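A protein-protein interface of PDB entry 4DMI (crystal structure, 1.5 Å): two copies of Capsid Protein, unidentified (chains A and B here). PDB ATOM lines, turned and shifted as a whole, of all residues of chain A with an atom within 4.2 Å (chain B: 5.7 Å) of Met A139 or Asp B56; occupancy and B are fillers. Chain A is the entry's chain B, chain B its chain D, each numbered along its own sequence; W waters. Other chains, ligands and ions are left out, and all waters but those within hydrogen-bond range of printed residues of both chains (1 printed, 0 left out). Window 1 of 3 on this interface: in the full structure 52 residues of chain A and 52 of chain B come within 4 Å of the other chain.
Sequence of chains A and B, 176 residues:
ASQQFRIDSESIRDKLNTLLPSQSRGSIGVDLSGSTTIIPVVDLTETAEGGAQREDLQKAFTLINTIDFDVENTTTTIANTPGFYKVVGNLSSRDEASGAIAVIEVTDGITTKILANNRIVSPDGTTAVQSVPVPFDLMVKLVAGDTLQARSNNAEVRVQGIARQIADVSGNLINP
OE2 of Glu A55 lies within salt-bridge range of NZ of Lys A59, at 3.8 Å.
N of Tyr A85 lies within hydrogen-bond range of O of Val A140.
The side-chain carboxylate (OD1) of Asp B56 is in salt-bridge range of the guanidinium group (NE) of Arg B54.
OE1 of Glu A55 is in salt-bridge range of NE of Arg B54 (3.7 Å).
The side-chain carboxylate of Asp B56 is in salt-bridge range of the side-chain amino group of Lys A59 (2.9 Å).
O of Met A139 lies within hydrogen-bond range of N of Phe B61 (2.9 Å).
2 positions are printed for both chains.
Of the 8 pairs that touch across the chains among the printed residues, none has its exchanged pair printed and touching as well.
Water W1 lies within hydrogen-bond range of OE1 of Glu A55 and N of Asp B56.
Printed residues of chain B within 4 Å of Lys A59: Arg B54 and Asp B56.
Lys A86 touches none of the printed residues of chain B.
Of the printed residues of chain B, Met A139 touches Asp B56 (3.4 Å), Ala B60 (3.5 Å) and Phe B61 (2.9 Å).
Printed residues of chain B within 4 Å of Val A140: Phe B61 (3.3 Å).
Printed residues of chain A within 4 Å of Arg B54: Glu A55 (3.5 Å) and Lys A59 (3.6 Å).
Of the printed residues of chain A, Asp B56 touches Glu A55 (3.6 Å), Lys A59 (2.9 Å) and Met A139 (3.4 Å).
Of the printed residues of chain A, Ala B60 touches Met A139.
Of the printed residues of chain A, Phe B61 touches Met A139 and Val A140.
The nearest printed residue of chain A that does not touch Asp B56 is Val A140 (6.7 Å).
Of the 8 printed residues of chain B, 4 touch a printed residue of chain A.
Hydrophobic or aromatic side chains of chain B within 4 Å of the printed part of chain A: Ala B60 and Phe B61.
Among the printed residues, 8 pairs touch across the chains.
Among the printed residues, Asp or Glu carboxylates within 4 Å of a Lys or Arg side-chain nitrogen of the other chain: Glu A55 with Arg B54 and Lys A59 with Asp B56.
OE2 of Glu A55 touches CG of Asp B56 (3.6 Å).
Lys A59 touches Arg B54.
Met A139 touches Asp B56 (CG to O, 3.4 Å).
Met A139 touches Ala B60 (O to CA, 3.5 Å).
Val A140 touches Phe B61 (CA to O, 3.3 Å).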
ATOM      1  N   GLU A  55     -24.615 -10.384 -22.357  1.00  0.00           N
ATOM      2  CA  GLU A  55     -23.566 -10.318 -23.363  1.00  0.00           C
ATOM      3  C   GLU A  55     -23.850  -9.381 -24.534  1.00  0.00           C
ATOM      4  O   GLU A  55     -22.983  -8.628 -24.966  1.00  0.00           O
ATOM      5  CB  GLU A  55     -23.264 -11.737 -23.857  1.00  0.00           C
ATOM      6  CG  GLU A  55     -22.299 -11.808 -25.006  1.00  0.00           C
ATOM      7  CD  GLU A  55     -21.972 -13.239 -25.381  1.00  0.00           C
ATOM      8  OE1 GLU A  55     -22.189 -14.136 -24.539  1.00  0.00           O
ATOM      9  OE2 GLU A  55     -21.504 -13.463 -26.519  1.00  0.00           O
ATOM     10  N   LYS A  59     -21.456  -6.058 -25.262  1.00  0.00           N
ATOM     11  CA  LYS A  59     -20.674  -5.977 -26.497  1.00  0.00           C
ATOM     12  C   LYS A  59     -21.096  -4.847 -27.438  1.00  0.00           C
ATOM     13  O   LYS A  59     -20.594  -4.756 -28.564  1.00  0.00           O
ATOM     14  CB  LYS A  59     -20.718  -7.320 -27.236  1.00  0.00           C
ATOM     15  CG  LYS A  59     -20.049  -8.431 -26.435  1.00  0.00           C
ATOM     16  CD  LYS A  59     -20.199  -9.794 -27.096  1.00  0.00           C
ATOM     17  CE  LYS A  59     -19.352  -9.916 -28.337  1.00  0.00           C
ATOM     18  NZ  LYS A  59     -19.334 -11.361 -28.779  1.00  0.00           N
ATOM     19  N   TYR A  85     -10.962  -8.518 -29.143  1.00  0.00           N
ATOM     20  CA  TYR A  85     -11.599  -7.561 -30.035  1.00  0.00           C
ATOM     21  C   TYR A  85     -12.632  -8.226 -30.914  1.00  0.00           C
ATOM     22  O   TYR A  85     -12.370  -9.270 -31.510  1.00  0.00           O
ATOM     23  CB  TYR A  85     -10.545  -6.891 -30.926  1.00  0.00           C
ATOM     24  CG  TYR A  85      -9.512  -6.092 -30.161  1.00  0.00           C
ATOM     25  CD1 TYR A  85      -8.378  -6.711 -29.643  1.00  0.00           C
ATOM     26  CD2 TYR A  85      -9.669  -4.730 -29.953  1.00  0.00           C
ATOM     27  CE1 TYR A  85      -7.421  -5.990 -28.940  1.00  0.00           C
ATOM     28  CE2 TYR A  85      -8.714  -3.995 -29.243  1.00  0.00           C
ATOM     29  CZ  TYR A  85      -7.599  -4.638 -28.744  1.00  0.00           C
ATOM     30  OH  TYR A  85      -6.638  -3.942 -28.047  1.00  0.00           O
ATOM     31  N   LYS A  86     -13.810  -7.615 -31.012  1.00  0.00           N
ATOM     32  CA  LYS A  86     -14.807  -8.031 -31.990  1.00  0.00           C
ATOM     33  C   LYS A  86     -14.573  -7.174 -33.221  1.00  0.00           C
ATOM     34  O   LYS A  86     -14.399  -5.972 -33.125  1.00  0.00           O
ATOM     35  CB  LYS A  86     -16.217  -7.803 -31.450  1.00  0.00           C
ATOM     36  CG  LYS A  86     -17.303  -7.908 -32.515  1.00  0.00           C
ATOM     37  CD  LYS A  86     -18.692  -7.756 -31.893  1.00  0.00           C
ATOM     38  CE  LYS A  86     -19.771  -8.027 -32.924  1.00  0.00           C
ATOM     39  NZ  LYS A  86     -21.119  -8.148 -32.316  1.00  0.00           N
ATOM     40  N   LEU A 138     -15.621 -11.614 -36.511  1.00  0.00           N
ATOM     41  CA  LEU A 138     -14.546 -12.320 -35.835  1.00  0.00           C
ATOM     42  C   LEU A 138     -14.372 -11.863 -34.396  1.00  0.00           C
ATOM     43  O   LEU A 138     -14.620 -10.700 -34.057  1.00  0.00           O
ATOM     44  CB  LEU A 138     -13.235 -12.057 -36.579  1.00  0.00           C
ATOM     45  CG  LEU A 138     -13.132 -12.558 -38.017  1.00  0.00           C
ATOM     46  CD1 LEU A 138     -12.126 -11.739 -38.808  1.00  0.00           C
ATOM     47  CD2 LEU A 138     -12.684 -14.000 -37.981  1.00  0.00           C
ATOM     48  N   MET A 139     -13.964 -12.798 -33.550  1.00  0.00           N
ATOM     49  CA  MET A 139     -13.412 -12.469 -32.251  1.00  0.00           C
ATOM     50  C   MET A 139     -11.938 -12.811 -32.290  1.00  0.00           C
ATOM     51  O   MET A 139     -11.548 -13.970 -32.549  1.00  0.00           O
ATOM     52  CB  MET A 139     -14.091 -13.258 -31.132  1.00  0.00           C
ATOM     53  CG  MET A 139     -13.557 -12.957 -29.722  1.00  0.00           C
ATOM     54  SD  MET A 139     -14.004 -11.310 -29.115  1.00  0.00           S
ATOM     55  CE  MET A 139     -15.647 -11.204 -29.831  1.00  0.00           C
ATOM     56  N   VAL A 140     -11.108 -11.807 -32.019  1.00  0.00           N
ATOM     57  CA  VAL A 140      -9.657 -11.945 -32.083  1.00  0.00           C
ATOM     58  C   VAL A 140      -9.033 -11.571 -30.751  1.00  0.00           C
ATOM     59  O   VAL A 140      -9.371 -10.540 -30.162  1.00  0.00           O
ATOM     60  CB  VAL A 140      -9.070 -11.021 -33.162  1.00  0.00           C
ATOM     61  CG1 VAL A 140      -7.545 -11.124 -33.203  1.00  0.00           C
ATOM     62  CG2 VAL A 140      -9.668 -11.355 -34.519  1.00  0.00           C
ATOM     63  N   ARG B  54     -16.136 -16.496 -20.697  1.00  0.00           N
ATOM     64  CA  ARG B  54     -17.320 -16.499 -21.543  1.00  0.00           C
ATOM     65  C   ARG B  54     -16.999 -17.161 -22.888  1.00  0.00           C
ATOM     66  O   ARG B  54     -15.884 -17.037 -23.396  1.00  0.00           O
ATOM     67  CB  ARG B  54     -17.820 -15.070 -21.732  1.00  0.00           C
ATOM     68  CG  ARG B  54     -19.258 -14.982 -22.145  1.00  0.00           C
ATOM     69  CD  ARG B  54     -19.751 -13.546 -22.082  1.00  0.00           C
ATOM     70  NE  ARG B  54     -19.066 -12.749 -23.093  1.00  0.00           N
ATOM     71  CZ  ARG B  54     -19.115 -11.420 -23.160  1.00  0.00           C
ATOM     72  NH1 ARG B  54     -19.820 -10.726 -22.272  1.00  0.00           N
ATOM     73  NH2 ARG B  54     -18.464 -10.799 -24.135  1.00  0.00           N
ATOM     74  N   GLU B  55     -17.980 -17.854 -23.458  1.00  0.00           N
ATOM     75  CA  GLU B  55     -17.753 -18.669 -24.646  1.00  0.00           C
ATOM     76  C   GLU B  55     -17.155 -17.907 -25.837  1.00  0.00           C
ATOM     77  O   GLU B  55     -16.244 -18.411 -26.515  1.00  0.00           O
ATOM     78  CB  GLU B  55     -19.054 -19.367 -25.023  1.00  0.00           C
ATOM     79  CG  GLU B  55     -19.018 -20.129 -26.306  1.00  0.00           C
ATOM     80  CD  GLU B  55     -20.334 -20.811 -26.569  1.00  0.00           C
ATOM     81  OE1 GLU B  55     -21.131 -20.947 -25.612  1.00  0.00           O
ATOM     82  OE2 GLU B  55     -20.583 -21.211 -27.726  1.00  0.00           O
ATOM     83  N   ASP B  56     -17.630 -16.683 -26.072  1.00  0.00           N
ATOM     84  CA  ASP B  56     -17.135 -15.910 -27.204  1.00  0.00           C
ATOM     85  C   ASP B  56     -15.644 -15.595 -27.059  1.00  0.00           C
ATOM     86  O   ASP B  56     -14.902 -15.621 -28.040  1.00  0.00           O
ATOM     87  CB  ASP B  56     -17.964 -14.633 -27.416  1.00  0.00           C
ATOM     88  CG  ASP B  56     -17.908 -13.677 -26.235  1.00  0.00           C
ATOM     89  OD1 ASP B  56     -17.773 -14.128 -25.075  1.00  0.00           O
ATOM     90  OD2 ASP B  56     -18.010 -12.455 -26.474  1.00  0.00           O
ATOM     91  N   LEU B  57     -15.210 -15.294 -25.841  1.00  0.00           N
ATOM     92  CA  LEU B  57     -13.797 -15.070 -25.587  1.00  0.00           C
ATOM     93  C   LEU B  57     -13.006 -16.367 -25.682  1.00  0.00           C
ATOM     94  O   LEU B  57     -11.950 -16.397 -26.295  1.00  0.00           O
ATOM     95  CB  LEU B  57     -13.582 -14.429 -24.218  1.00  0.00           C
ATOM     96  CG  LEU B  57     -14.399 -13.175 -23.939  1.00  0.00           C
ATOM     97  CD1 LEU B  57     -14.105 -12.716 -22.521  1.00  0.00           C
ATOM     98  CD2 LEU B  57     -14.047 -12.093 -24.941  1.00  0.00           C
ATOM     99  N   GLN B  58     -13.522 -17.441 -25.091  1.00  0.00           N
ATOM    100  CA  GLN B  58     -12.807 -18.712 -25.096  1.00  0.00           C
ATOM    101  C   GLN B  58     -12.533 -19.203 -26.516  1.00  0.00           C
ATOM    102  O   GLN B  58     -11.517 -19.854 -26.745  1.00  0.00           O
ATOM    103  CB  GLN B  58     -13.568 -19.778 -24.295  1.00  0.00           C
ATOM    104  CG  GLN B  58     -12.829 -21.133 -24.177  1.00  0.00           C
ATOM    105  CD  GLN B  58     -13.194 -22.113 -25.280  1.00  0.00           C
ATOM    106  OE1 GLN B  58     -14.347 -22.187 -25.701  1.00  0.00           O
ATOM    107  NE2 GLN B  58     -12.213 -22.865 -25.753  1.00  0.00           N
ATOM    108  N   LYS B  59     -13.415 -18.877 -27.455  1.00  0.00           N
ATOM    109  CA  LYS B  59     -13.303 -19.365 -28.828  1.00  0.00           C
ATOM    110  C   LYS B  59     -12.534 -18.436 -29.760  1.00  0.00           C
ATOM    111  O   LYS B  59     -12.475 -18.667 -30.967  1.00  0.00           O
ATOM    112  CB  LYS B  59     -14.698 -19.663 -29.412  1.00  0.00           C
ATOM    113  CG  LYS B  59     -15.410 -20.781 -28.665  1.00  0.00           C
ATOM    114  CD  LYS B  59     -16.831 -20.987 -29.164  1.00  0.00           C
ATOM    115  CE  LYS B  59     -16.864 -21.569 -30.558  1.00  0.00           C
ATOM    116  NZ  LYS B  59     -18.261 -21.998 -30.922  1.00  0.00           N
ATOM    117  N   ALA B  60     -11.916 -17.394 -29.208  1.00  0.00           N
ATOM    118  CA  ALA B  60     -11.248 -16.381 -30.028  1.00  0.00           C
ATOM    119  C   ALA B  60     -10.100 -16.927 -30.876  1.00  0.00           C
ATOM    120  O   ALA B  60      -9.376 -17.823 -30.453  1.00  0.00           O
ATOM    121  CB  ALA B  60     -10.720 -15.252 -29.126  1.00  0.00           C
ATOM    122  N   PHE B  61      -9.917 -16.347 -32.057  1.00  0.00           N
ATOM    123  CA  PHE B  61      -8.732 -16.639 -32.872  1.00  0.00           C
ATOM    124  C   PHE B  61      -7.529 -15.791 -32.466  1.00  0.00           C
ATOM    125  O   PHE B  61      -7.651 -14.614 -32.120  1.00  0.00           O
ATOM    126  CB  PHE B  61      -9.063 -16.393 -34.346  1.00  0.00           C
ATOM    127  CG  PHE B  61     -10.007 -17.396 -34.922  1.00  0.00           C
ATOM    128  CD1 PHE B  61      -9.550 -18.597 -35.412  1.00  0.00           C
ATOM    129  CD2 PHE B  61     -11.364 -17.120 -34.987  1.00  0.00           C
ATOM    130  CE1 PHE B  61     -10.418 -19.532 -35.954  1.00  0.00           C
ATOM    131  CE2 PHE B  61     -12.251 -18.063 -35.541  1.00  0.00           C
ATOM    132  CZ  PHE B  61     -11.771 -19.262 -36.014  1.00  0.00           C
HETATM  133  O   HOH W   1     -20.673 -16.019 -25.438  1.00  0.00           O
